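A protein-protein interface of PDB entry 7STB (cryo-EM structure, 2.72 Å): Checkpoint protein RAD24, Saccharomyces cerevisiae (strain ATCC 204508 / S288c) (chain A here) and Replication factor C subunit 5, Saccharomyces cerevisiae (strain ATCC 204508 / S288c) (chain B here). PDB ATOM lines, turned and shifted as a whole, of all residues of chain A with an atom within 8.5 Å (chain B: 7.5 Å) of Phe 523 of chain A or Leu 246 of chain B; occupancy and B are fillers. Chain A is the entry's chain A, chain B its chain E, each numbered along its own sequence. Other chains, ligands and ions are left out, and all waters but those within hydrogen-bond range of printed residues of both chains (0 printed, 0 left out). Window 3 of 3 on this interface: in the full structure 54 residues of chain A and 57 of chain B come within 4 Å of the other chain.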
ATOM      1  N   CYS A 494     -12.807   3.204 -13.483  1.00  0.00           N
ATOM      2  CA  CYS A 494     -13.805   2.145 -13.360  1.00  0.00           C
ATOM      3  C   CYS A 494     -13.603   1.350 -12.075  1.00  0.00           C
ATOM      4  O   CYS A 494     -14.578   0.948 -11.424  1.00  0.00           O
ATOM      5  CB  CYS A 494     -13.758   1.228 -14.581  1.00  0.00           C
ATOM      6  SG  CYS A 494     -12.246   0.271 -14.740  1.00  0.00           S
ATOM      7  N   GLN A 495     -12.346   1.119 -11.686  1.00  0.00           N
ATOM      8  CA  GLN A 495     -12.080   0.432 -10.428  1.00  0.00           C
ATOM      9  C   GLN A 495     -12.596   1.241  -9.247  1.00  0.00           C
ATOM     10  O   GLN A 495     -13.158   0.680  -8.302  1.00  0.00           O
ATOM     11  CB  GLN A 495     -10.582   0.168 -10.282  1.00  0.00           C
ATOM     12  CG  GLN A 495     -10.131  -1.171 -10.843  1.00  0.00           C
ATOM     13  CD  GLN A 495      -8.622  -1.293 -10.924  1.00  0.00           C
ATOM     14  OE1 GLN A 495      -7.913  -0.294 -11.032  1.00  0.00           O
ATOM     15  NE2 GLN A 495      -8.125  -2.523 -10.870  1.00  0.00           N
ATOM     16  N   LYS A 498     -16.394   0.883  -9.105  1.00  0.00           N
ATOM     17  CA  LYS A 498     -16.772  -0.393  -8.509  1.00  0.00           C
ATOM     18  C   LYS A 498     -16.476  -0.420  -7.015  1.00  0.00           C
ATOM     19  O   LYS A 498     -17.225  -1.034  -6.247  1.00  0.00           O
ATOM     20  CB  LYS A 498     -16.058  -1.544  -9.215  1.00  0.00           C
ATOM     21  CG  LYS A 498     -16.664  -2.905  -8.911  1.00  0.00           C
ATOM     22  CD  LYS A 498     -16.698  -3.801 -10.136  1.00  0.00           C
ATOM     23  CE  LYS A 498     -17.501  -5.064  -9.868  1.00  0.00           C
ATOM     24  NZ  LYS A 498     -17.813  -5.808 -11.117  1.00  0.00           N
ATOM     25  N   LYS A 499     -15.392   0.229  -6.586  1.00  0.00           N
ATOM     26  CA  LYS A 499     -15.092   0.310  -5.160  1.00  0.00           C
ATOM     27  C   LYS A 499     -16.183   1.066  -4.417  1.00  0.00           C
ATOM     28  O   LYS A 499     -16.608   0.650  -3.334  1.00  0.00           O
ATOM     29  CB  LYS A 499     -13.736   0.983  -4.949  1.00  0.00           C
ATOM     30  CG  LYS A 499     -13.359   1.173  -3.488  1.00  0.00           C
ATOM     31  CD  LYS A 499     -11.916   1.627  -3.344  1.00  0.00           C
ATOM     32  CE  LYS A 499     -11.542   1.841  -1.886  1.00  0.00           C
ATOM     33  NZ  LYS A 499     -10.127   2.276  -1.733  1.00  0.00           N
ATOM     34  N   TYR A 501     -19.309   1.334  -5.361  1.00  0.00           N
ATOM     35  CA  TYR A 501     -20.494   0.482  -5.357  1.00  0.00           C
ATOM     36  C   TYR A 501     -20.393  -0.590  -4.276  1.00  0.00           C
ATOM     37  O   TYR A 501     -21.345  -0.820  -3.519  1.00  0.00           O
ATOM     38  CB  TYR A 501     -20.684  -0.160  -6.732  1.00  0.00           C
ATOM     39  CG  TYR A 501     -21.476  -1.447  -6.696  1.00  0.00           C
ATOM     40  CD1 TYR A 501     -22.846  -1.436  -6.464  1.00  0.00           C
ATOM     41  CD2 TYR A 501     -20.855  -2.674  -6.891  1.00  0.00           C
ATOM     42  CE1 TYR A 501     -23.573  -2.610  -6.429  1.00  0.00           C
ATOM     43  CE2 TYR A 501     -21.575  -3.853  -6.858  1.00  0.00           C
ATOM     44  CZ  TYR A 501     -22.934  -3.816  -6.627  1.00  0.00           C
ATOM     45  OH  TYR A 501     -23.655  -4.987  -6.593  1.00  0.00           O
ATOM     46  N   ILE A 502     -19.237  -1.252  -4.187  1.00  0.00           N
ATOM     47  CA  ILE A 502     -19.062  -2.319  -3.207  1.00  0.00           C
ATOM     48  C   ILE A 502     -19.125  -1.762  -1.791  1.00  0.00           C
ATOM     49  O   ILE A 502     -19.723  -2.373  -0.897  1.00  0.00           O
ATOM     50  CB  ILE A 502     -17.739  -3.065  -3.464  1.00  0.00           C
ATOM     51  CG1 ILE A 502     -17.822  -3.853  -4.773  1.00  0.00           C
ATOM     52  CG2 ILE A 502     -17.418  -3.994  -2.301  1.00  0.00           C
ATOM     53  CD1 ILE A 502     -16.476  -4.284  -5.316  1.00  0.00           C
ATOM     54  N   TYR A 505     -22.725  -1.030  -0.950  1.00  0.00           N
ATOM     55  CA  TYR A 505     -23.456  -2.272  -0.719  1.00  0.00           C
ATOM     56  C   TYR A 505     -23.125  -2.857   0.647  1.00  0.00           C
ATOM     57  O   TYR A 505     -24.021  -3.310   1.372  1.00  0.00           O
ATOM     58  CB  TYR A 505     -23.138  -3.280  -1.824  1.00  0.00           C
ATOM     59  CG  TYR A 505     -23.489  -4.706  -1.465  1.00  0.00           C
ATOM     60  CD1 TYR A 505     -24.813  -5.114  -1.370  1.00  0.00           C
ATOM     61  CD2 TYR A 505     -22.496  -5.646  -1.220  1.00  0.00           C
ATOM     62  CE1 TYR A 505     -25.138  -6.417  -1.043  1.00  0.00           C
ATOM     63  CE2 TYR A 505     -22.811  -6.950  -0.893  1.00  0.00           C
ATOM     64  CZ  TYR A 505     -24.134  -7.330  -0.805  1.00  0.00           C
ATOM     65  OH  TYR A 505     -24.453  -8.629  -0.478  1.00  0.00           O
ATOM     66  N   LEU A 506     -21.843  -2.861   1.018  1.00  0.00           N
ATOM     67  CA  LEU A 506     -21.454  -3.387   2.322  1.00  0.00           C
ATOM     68  C   LEU A 506     -22.033  -2.542   3.451  1.00  0.00           C
ATOM     69  O   LEU A 506     -22.502  -3.080   4.460  1.00  0.00           O
ATOM     70  CB  LEU A 506     -19.929  -3.450   2.430  1.00  0.00           C
ATOM     71  CG  LEU A 506     -19.230  -4.510   1.573  1.00  0.00           C
ATOM     72  CD1 LEU A 506     -17.721  -4.407   1.730  1.00  0.00           C
ATOM     73  CD2 LEU A 506     -19.710  -5.910   1.932  1.00  0.00           C
ATOM     74  N   MET A 520     -15.034  -7.303   0.322  1.00  0.00           N
ATOM     75  CA  MET A 520     -13.671  -6.814   0.163  1.00  0.00           C
ATOM     76  C   MET A 520     -12.744  -7.939  -0.286  1.00  0.00           C
ATOM     77  O   MET A 520     -11.884  -7.744  -1.144  1.00  0.00           O
ATOM     78  CB  MET A 520     -13.163  -6.206   1.471  1.00  0.00           C
ATOM     79  N   ASP A 521     -12.926  -9.122   0.305  1.00  0.00           N
ATOM     80  CA  ASP A 521     -12.090 -10.263  -0.056  1.00  0.00           C
ATOM     81  C   ASP A 521     -12.307 -10.666  -1.510  1.00  0.00           C
ATOM     82  O   ASP A 521     -11.354 -11.024  -2.211  1.00  0.00           O
ATOM     83  CB  ASP A 521     -12.381 -11.440   0.875  1.00  0.00           C
ATOM     84  CG  ASP A 521     -12.151 -11.100   2.333  1.00  0.00           C
ATOM     85  OD1 ASP A 521     -11.503 -10.067   2.610  1.00  0.00           O
ATOM     86  OD2 ASP A 521     -12.615 -11.864   3.205  1.00  0.00           O
ATOM     87  N   LYS A 522     -13.555 -10.616  -1.979  1.00  0.00           N
ATOM     88  CA  LYS A 522     -13.844 -11.012  -3.354  1.00  0.00           C
ATOM     89  C   LYS A 522     -13.127 -10.110  -4.350  1.00  0.00           C
ATOM     90  O   LYS A 522     -12.605 -10.585  -5.365  1.00  0.00           O
ATOM     91  CB  LYS A 522     -15.352 -10.986  -3.602  1.00  0.00           C
ATOM     92  CG  LYS A 522     -16.163 -11.813  -2.616  1.00  0.00           C
ATOM     93  CD  LYS A 522     -17.654 -11.672  -2.874  1.00  0.00           C
ATOM     94  CE  LYS A 522     -18.473 -12.451  -1.856  1.00  0.00           C
ATOM     95  NZ  LYS A 522     -19.936 -12.301  -2.086  1.00  0.00           N
ATOM     96  N   PHE A 523     -13.093  -8.807  -4.080  1.00  0.00           N
ATOM     97  CA  PHE A 523     -12.493  -7.815  -4.967  1.00  0.00           C
ATOM     98  C   PHE A 523     -11.456  -6.993  -4.213  1.00  0.00           C
ATOM     99  O   PHE A 523     -11.438  -5.762  -4.265  1.00  0.00           O
ATOM    100  CB  PHE A 523     -13.564  -6.912  -5.570  1.00  0.00           C
ATOM    101  CG  PHE A 523     -14.693  -7.661  -6.217  1.00  0.00           C
ATOM    102  CD1 PHE A 523     -14.500  -8.337  -7.410  1.00  0.00           C
ATOM    103  CD2 PHE A 523     -15.948  -7.690  -5.633  1.00  0.00           C
ATOM    104  CE1 PHE A 523     -15.536  -9.029  -8.007  1.00  0.00           C
ATOM    105  CE2 PHE A 523     -16.988  -8.379  -6.226  1.00  0.00           C
ATOM    106  CZ  PHE A 523     -16.782  -9.049  -7.415  1.00  0.00           C
ATOM    107  N   SER A 524     -10.569  -7.683  -3.490  1.00  0.00           N
ATOM    108  CA  SER A 524      -9.536  -6.989  -2.729  1.00  0.00           C
ATOM    109  C   SER A 524      -8.677  -6.106  -3.625  1.00  0.00           C
ATOM    110  O   SER A 524      -8.205  -5.051  -3.185  1.00  0.00           O
ATOM    111  CB  SER A 524      -8.660  -8.003  -1.992  1.00  0.00           C
ATOM    112  OG  SER A 524      -8.002  -8.865  -2.902  1.00  0.00           O
ATOM    113  N   ASP A 525      -8.461  -6.514  -4.877  1.00  0.00           N
ATOM    114  CA  ASP A 525      -7.668  -5.697  -5.789  1.00  0.00           C
ATOM    115  C   ASP A 525      -8.317  -4.337  -6.010  1.00  0.00           C
ATOM    116  O   ASP A 525      -7.633  -3.306  -6.008  1.00  0.00           O
ATOM    117  CB  ASP A 525      -7.486  -6.426  -7.121  1.00  0.00           C
ATOM    118  CG  ASP A 525      -6.695  -7.711  -6.978  1.00  0.00           C
ATOM    119  OD1 ASP A 525      -6.112  -7.934  -5.896  1.00  0.00           O
ATOM    120  OD2 ASP A 525      -6.656  -8.497  -7.947  1.00  0.00           O
ATOM    121  N   ILE A 526      -9.637  -4.313  -6.201  1.00  0.00           N
ATOM    122  CA  ILE A 526     -10.336  -3.043  -6.372  1.00  0.00           C
ATOM    123  C   ILE A 526     -10.265  -2.221  -5.093  1.00  0.00           C
ATOM    124  O   ILE A 526     -10.139  -0.991  -5.135  1.00  0.00           O
ATOM    125  CB  ILE A 526     -11.793  -3.294  -6.806  1.00  0.00           C
ATOM    126  CG1 ILE A 526     -11.825  -3.945  -8.193  1.00  0.00           C
ATOM    127  CG2 ILE A 526     -12.578  -1.988  -6.799  1.00  0.00           C
ATOM    128  CD1 ILE A 526     -13.202  -4.409  -8.627  1.00  0.00           C
ATOM    129  N   MET A 527     -10.342  -2.881  -3.935  1.00  0.00           N
ATOM    130  CA  MET A 527     -10.279  -2.169  -2.664  1.00  0.00           C
ATOM    131  C   MET A 527      -8.949  -1.452  -2.472  1.00  0.00           C
ATOM    132  O   MET A 527      -8.881  -0.496  -1.692  1.00  0.00           O
ATOM    133  CB  MET A 527     -10.505  -3.144  -1.507  1.00  0.00           C
ATOM    134  CG  MET A 527     -11.894  -3.765  -1.469  1.00  0.00           C
ATOM    135  SD  MET A 527     -13.211  -2.551  -1.262  1.00  0.00           S
ATOM    136  CE  MET A 527     -13.830  -2.435  -2.938  1.00  0.00           C
ATOM    137  N   LYS A 528      -7.896  -1.886  -3.163  1.00  0.00           N
ATOM    138  CA  LYS A 528      -6.574  -1.292  -3.009  1.00  0.00           C
ATOM    139  C   LYS A 528      -6.383  -0.034  -3.846  1.00  0.00           C
ATOM    140  O   LYS A 528      -5.321   0.591  -3.757  1.00  0.00           O
ATOM    141  CB  LYS A 528      -5.497  -2.317  -3.375  1.00  0.00           C
ATOM    142  CG  LYS A 528      -5.306  -3.409  -2.333  1.00  0.00           C
ATOM    143  CD  LYS A 528      -4.056  -4.233  -2.603  1.00  0.00           C
ATOM    144  CE  LYS A 528      -4.154  -4.987  -3.921  1.00  0.00           C
ATOM    145  NZ  LYS A 528      -3.024  -5.937  -4.106  1.00  0.00           N
ATOM    146  N   VAL A 529      -7.372   0.352  -4.646  1.00  0.00           N
ATOM    147  CA  VAL A 529      -7.262   1.545  -5.480  1.00  0.00           C
ATOM    148  C   VAL A 529      -7.580   2.765  -4.627  1.00  0.00           C
ATOM    149  O   VAL A 529      -8.677   2.877  -4.069  1.00  0.00           O
ATOM    150  CB  VAL A 529      -8.198   1.457  -6.695  1.00  0.00           C
ATOM    151  CG1 VAL A 529      -8.104   2.724  -7.536  1.00  0.00           C
ATOM    152  CG2 VAL A 529      -7.866   0.230  -7.530  1.00  0.00           C
ATOM    153  N   TRP B   4      -2.281  -5.296 -14.716  1.00  0.00           N
ATOM    154  CA  TRP B   4      -1.983  -6.678 -15.072  1.00  0.00           C
ATOM    155  C   TRP B   4      -0.765  -6.789 -15.980  1.00  0.00           C
ATOM    156  O   TRP B   4      -0.171  -7.868 -16.071  1.00  0.00           O
ATOM    157  CB  TRP B   4      -3.198  -7.319 -15.746  1.00  0.00           C
ATOM    158  CG  TRP B   4      -4.423  -7.341 -14.879  1.00  0.00           C
ATOM    159  CD1 TRP B   4      -4.493  -7.045 -13.548  1.00  0.00           C
ATOM    160  CD2 TRP B   4      -5.756  -7.677 -15.284  1.00  0.00           C
ATOM    161  NE1 TRP B   4      -5.785  -7.175 -13.100  1.00  0.00           N
ATOM    162  CE2 TRP B   4      -6.580  -7.563 -14.146  1.00  0.00           C
ATOM    163  CE3 TRP B   4      -6.332  -8.063 -16.497  1.00  0.00           C
ATOM    164  CZ2 TRP B   4      -7.948  -7.820 -14.187  1.00  0.00           C
ATOM    165  CZ3 TRP B   4      -7.691  -8.319 -16.534  1.00  0.00           C
ATOM    166  CH2 TRP B   4      -8.483  -8.196 -15.386  1.00  0.00           C
ATOM    167  N   GLU B 209      -7.567 -14.475 -12.836  1.00  0.00           N
ATOM    168  CA  GLU B 209      -8.280 -13.337 -12.270  1.00  0.00           C
ATOM    169  C   GLU B 209      -9.733 -13.652 -11.939  1.00  0.00           C
ATOM    170  O   GLU B 209     -10.455 -12.758 -11.486  1.00  0.00           O
ATOM    171  CB  GLU B 209      -8.219 -12.149 -13.234  1.00  0.00           C
ATOM    172  CG  GLU B 209      -6.935 -11.337 -13.141  1.00  0.00           C
ATOM    173  CD  GLU B 209      -6.861 -10.504 -11.876  1.00  0.00           C
ATOM    174  OE1 GLU B 209      -7.921 -10.040 -11.404  1.00  0.00           O
ATOM    175  OE2 GLU B 209      -5.743 -10.312 -11.353  1.00  0.00           O
ATOM    176  N   ARG B 210     -10.176 -14.892 -12.150  1.00  0.00           N
ATOM    177  CA  ARG B 210     -11.550 -15.294 -11.851  1.00  0.00           C
ATOM    178  C   ARG B 210     -12.550 -14.446 -12.633  1.00  0.00           C
ATOM    179  O   ARG B 210     -13.611 -14.076 -12.125  1.00  0.00           O
ATOM    180  CB  ARG B 210     -11.829 -15.217 -10.349  1.00  0.00           C
ATOM    181  CG  ARG B 210     -10.911 -16.086  -9.504  1.00  0.00           C
ATOM    182  CD  ARG B 210     -11.134 -15.849  -8.019  1.00  0.00           C
ATOM    183  NE  ARG B 210     -10.203 -16.615  -7.197  1.00  0.00           N
ATOM    184  CZ  ARG B 210     -10.173 -16.585  -5.871  1.00  0.00           C
ATOM    185  NH1 ARG B 210     -11.014 -15.838  -5.176  1.00  0.00           N
ATOM    186  NH2 ARG B 210      -9.276 -17.326  -5.227  1.00  0.00           N
ATOM    187  N   ILE B 211     -12.209 -14.136 -13.880  1.00  0.00           N
ATOM    188  CA  ILE B 211     -13.066 -13.366 -14.774  1.00  0.00           C
ATOM    189  C   ILE B 211     -13.794 -14.332 -15.695  1.00  0.00           C
ATOM    190  O   ILE B 211     -13.241 -15.364 -16.097  1.00  0.00           O
ATOM    191  CB  ILE B 211     -12.248 -12.339 -15.579  1.00  0.00           C
ATOM    192  CG1 ILE B 211     -11.513 -11.377 -14.640  1.00  0.00           C
ATOM    193  CG2 ILE B 211     -13.148 -11.571 -16.538  1.00  0.00           C
ATOM    194  CD1 ILE B 211     -12.422 -10.561 -13.744  1.00  0.00           C
ATOM    195  N   GLN B 212     -15.037 -14.000 -16.031  1.00  0.00           N
ATOM    196  CA  GLN B 212     -15.886 -14.880 -16.822  1.00  0.00           C
ATOM    197  C   GLN B 212     -15.688 -14.627 -18.310  1.00  0.00           C
ATOM    198  O   GLN B 212     -15.563 -13.480 -18.748  1.00  0.00           O
ATOM    199  CB  GLN B 212     -17.356 -14.680 -16.452  1.00  0.00           C
ATOM    200  CG  GLN B 212     -17.650 -14.855 -14.971  1.00  0.00           C
ATOM    201  CD  GLN B 212     -17.271 -16.231 -14.459  1.00  0.00           C
ATOM    202  OE1 GLN B 212     -17.609 -17.247 -15.067  1.00  0.00           O
ATOM    203  NE2 GLN B 212     -16.564 -16.271 -13.335  1.00  0.00           N
ATOM    204  N   LEU B 213     -15.659 -15.711 -19.081  1.00  0.00           N
ATOM    205  CA  LEU B 213     -15.545 -15.653 -20.531  1.00  0.00           C
ATOM    206  C   LEU B 213     -16.579 -16.576 -21.156  1.00  0.00           C
ATOM    207  O   LEU B 213     -16.982 -17.578 -20.559  1.00  0.00           O
ATOM    208  CB  LEU B 213     -14.141 -16.053 -21.007  1.00  0.00           C
ATOM    209  CG  LEU B 213     -13.156 -14.914 -21.277  1.00  0.00           C
ATOM    210  CD1 LEU B 213     -11.762 -15.471 -21.508  1.00  0.00           C
ATOM    211  CD2 LEU B 213     -13.600 -14.080 -22.470  1.00  0.00           C
ATOM    212  N   GLU B 238      -7.988  -5.813 -19.733  1.00  0.00           N
ATOM    213  CA  GLU B 238      -8.402  -5.353 -18.412  1.00  0.00           C
ATOM    214  C   GLU B 238      -9.515  -4.319 -18.516  1.00  0.00           C
ATOM    215  O   GLU B 238     -10.482  -4.352 -17.743  1.00  0.00           O
ATOM    216  CB  GLU B 238      -7.205  -4.774 -17.659  1.00  0.00           C
ATOM    217  CG  GLU B 238      -7.447  -4.585 -16.171  1.00  0.00           C
ATOM    218  CD  GLU B 238      -6.199  -4.150 -15.426  1.00  0.00           C
ATOM    219  OE1 GLU B 238      -5.096  -4.608 -15.789  1.00  0.00           O
ATOM    220  OE2 GLU B 238      -6.323  -3.349 -14.476  1.00  0.00           O
ATOM    221  N   MET B 240     -11.766  -3.945 -20.914  1.00  0.00           N
ATOM    222  CA  MET B 240     -13.004  -4.623 -21.282  1.00  0.00           C
ATOM    223  C   MET B 240     -13.581  -5.396 -20.104  1.00  0.00           C
ATOM    224  O   MET B 240     -14.791  -5.352 -19.857  1.00  0.00           O
ATOM    225  CB  MET B 240     -12.752  -5.568 -22.458  1.00  0.00           C
ATOM    226  CG  MET B 240     -12.397  -4.872 -23.758  1.00  0.00           C
ATOM    227  SD  MET B 240     -12.030  -6.049 -25.072  1.00  0.00           S
ATOM    228  CE  MET B 240     -13.659  -6.724 -25.389  1.00  0.00           C
ATOM    229  N   ALA B 241     -12.732  -6.111 -19.364  1.00  0.00           N
ATOM    230  CA  ALA B 241     -13.222  -6.894 -18.236  1.00  0.00           C
ATOM    231  C   ALA B 241     -13.861  -6.000 -17.183  1.00  0.00           C
ATOM    232  O   ALA B 241     -14.928  -6.322 -16.647  1.00  0.00           O
ATOM    233  CB  ALA B 241     -12.081  -7.708 -17.628  1.00  0.00           C
ATOM    234  N   LEU B 242     -13.227  -4.867 -16.875  1.00  0.00           N
ATOM    235  CA  LEU B 242     -13.774  -3.975 -15.857  1.00  0.00           C
ATOM    236  C   LEU B 242     -15.036  -3.278 -16.350  1.00  0.00           C
ATOM    237  O   LEU B 242     -15.988  -3.094 -15.583  1.00  0.00           O
ATOM    238  CB  LEU B 242     -12.719  -2.952 -15.441  1.00  0.00           C
ATOM    239  CG  LEU B 242     -11.441  -3.542 -14.836  1.00  0.00           C
ATOM    240  CD1 LEU B 242     -10.355  -2.485 -14.708  1.00  0.00           C
ATOM    241  CD2 LEU B 242     -11.732  -4.170 -13.485  1.00  0.00           C
ATOM    242  N   ASN B 243     -15.065  -2.882 -17.625  1.00  0.00           N
ATOM    243  CA  ASN B 243     -16.232  -2.185 -18.157  1.00  0.00           C
ATOM    244  C   ASN B 243     -17.464  -3.082 -18.152  1.00  0.00           C
ATOM    245  O   ASN B 243     -18.571  -2.628 -17.838  1.00  0.00           O
ATOM    246  CB  ASN B 243     -15.944  -1.682 -19.570  1.00  0.00           C
ATOM    247  CG  ASN B 243     -15.217  -0.352 -19.580  1.00  0.00           C
ATOM    248  OD1 ASN B 243     -14.836   0.170 -18.532  1.00  0.00           O
ATOM    249  ND2 ASN B 243     -15.021   0.207 -20.769  1.00  0.00           N
ATOM    250  N   ASN B 244     -17.293  -4.358 -18.497  1.00  0.00           N
ATOM    251  CA  ASN B 244     -18.399  -5.300 -18.584  1.00  0.00           C
ATOM    252  C   ASN B 244     -18.718  -5.959 -17.246  1.00  0.00           C
ATOM    253  O   ASN B 244     -19.295  -7.052 -17.227  1.00  0.00           O
ATOM    254  CB  ASN B 244     -18.093  -6.372 -19.634  1.00  0.00           C
ATOM    255  CG  ASN B 244     -17.751  -5.782 -20.989  1.00  0.00           C
ATOM    256  OD1 ASN B 244     -16.796  -6.206 -21.638  1.00  0.00           O
ATOM    257  ND2 ASN B 244     -18.536  -4.804 -21.427  1.00  0.00           N
ATOM    258  N   GLU B 245     -18.357  -5.323 -16.133  1.00  0.00           N
ATOM    259  CA  GLU B 245     -18.618  -5.868 -14.801  1.00  0.00           C
ATOM    260  C   GLU B 245     -17.987  -7.248 -14.641  1.00  0.00           C
ATOM    261  O   GLU B 245     -18.602  -8.177 -14.112  1.00  0.00           O
ATOM    262  CB  GLU B 245     -20.120  -5.924 -14.516  1.00  0.00           C
ATOM    263  CG  GLU B 245     -20.841  -4.599 -14.718  1.00  0.00           C
ATOM    264  CD  GLU B 245     -20.244  -3.478 -13.891  1.00  0.00           C
ATOM    265  OE1 GLU B 245     -20.016  -3.686 -12.680  1.00  0.00           O
ATOM    266  OE2 GLU B 245     -20.002  -2.388 -14.451  1.00  0.00           O
ATOM    267  N   LEU B 246     -16.744  -7.383 -15.102  1.00  0.00           N
ATOM    268  CA  LEU B 246     -16.005  -8.642 -15.002  1.00  0.00           C
ATOM    269  C   LEU B 246     -16.758  -9.778 -15.689  1.00  0.00           C
ATOM    270  O   LEU B 246     -16.816 -10.902 -15.186  1.00  0.00           O
ATOM    271  CB  LEU B 246     -15.715  -8.989 -13.542  1.00  0.00           C
ATOM    272  CG  LEU B 246     -15.072  -7.881 -12.705  1.00  0.00           C
ATOM    273  CD1 LEU B 246     -14.617  -8.423 -11.358  1.00  0.00           C
ATOM    274  CD2 LEU B 246     -13.911  -7.230 -13.443  1.00  0.00           C
ATOM    275  N   ALA B 247     -17.342  -9.482 -16.851  1.00  0.00           N
ATOM    276  CA  ALA B 247     -18.074 -10.488 -17.620  1.00  0.00           C
ATOM    277  C   ALA B 247     -17.848 -10.186 -19.099  1.00  0.00           C
ATOM    278  O   ALA B 247     -18.547  -9.347 -19.677  1.00  0.00           O
ATOM    279  CB  ALA B 247     -19.555 -10.482 -17.266  1.00  0.00           C
ATOM    280  N   LEU B 248     -16.881 -10.872 -19.700  1.00  0.00           N
ATOM    281  CA  LEU B 248     -16.549 -10.659 -21.104  1.00  0.00           C
ATOM    282  C   LEU B 248     -17.466 -11.504 -21.978  1.00  0.00           C
ATOM    283  O   LEU B 248     -17.434 -12.738 -21.912  1.00  0.00           O
ATOM    284  CB  LEU B 248     -15.086 -11.009 -21.362  1.00  0.00           C
ATOM    285  CG  LEU B 248     -14.055  -9.979 -20.896  1.00  0.00           C
ATOM    286  CD1 LEU B 248     -12.655 -10.570 -20.937  1.00  0.00           C
ATOM    287  CD2 LEU B 248     -14.130  -8.716 -21.739  1.00  0.00           C
ATOM    288  N   LYS B 249     -18.280 -10.843 -22.795  1.00  0.00           N
ATOM    289  CA  LYS B 249     -19.206 -11.512 -23.696  1.00  0.00           C
ATOM    290  C   LYS B 249     -18.679 -11.472 -25.127  1.00  0.00           C
ATOM    291  O   LYS B 249     -17.730 -10.755 -25.452  1.00  0.00           O
ATOM    292  CB  LYS B 249     -20.591 -10.860 -23.619  1.00  0.00           C
ATOM    293  CG  LYS B 249     -21.270 -11.010 -22.265  1.00  0.00           C
ATOM    294  CD  LYS B 249     -22.543 -10.180 -22.178  1.00  0.00           C
ATOM    295  CE  LYS B 249     -22.239  -8.696 -22.035  1.00  0.00           C
ATOM    296  NZ  LYS B 249     -23.474  -7.890 -21.838  1.00  0.00           N
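NZ of Lys 498 of chain A is in salt-bridge range of OE1 of Glu 245 of chain B.
The backbone NH (N) of Leu 246 of chain B is in hydrogen-bond range of the backbone carbonyl oxygen (O) of Ala 241 of chain B.
Among the printed residues, merely in contact across the chains: Cys 494 of chain A with Leu 242 of chain B, Lys 498 of chain A with Leu 246 of chain B, Phe 523 of chain A with Leu 246 of chain B and Asp 525 of chain A with Glu 209 of chain B.
Of the printed residues of chain B, Lys 498 of chain A touches Glu 245 (3.4 Å) and Leu 246 (3.8 Å).
Lys 499 of chain A touches none of the printed residues of chain B.
Tyr 505 of chain A touches none of the printed residues of chain B.
Of chain B, only Leu 246 (3.5 Å) comes within 4 Å of Phe 523 of chain A.
Printed residues of chain A within 4 Å of Glu 209 of chain B: Asp 525.
Of chain A, only Lys 498 and Phe 523 come within 4 Å of Leu 246 of chain B.
No residue of chain A comes within 4 Å of Ala 247 of chain B.
The nearest residue of chain B that does not touch Phe 523 of chain A is Ile 211 of chain B (6.7 Å).
The nearest residue of chain A that does not touch Leu 246 of chain B is Ile 526 of chain A (5.1 Å).
Hydrophobic or aromatic side chains of chain B that line the printed part of chain A: Leu 242 and Leu 246.
Of the 18 printed residues of chain A, 4 touch a printed residue of chain B.
Among the printed residues, 5 pairs touch across the chains.
Among the printed residues, Asp or Glu carboxylates within 4 Å of a Lys or Arg side-chain nitrogen of the other chain: Lys 498 of chain A with Glu 245 of chain B (3.4 Å).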
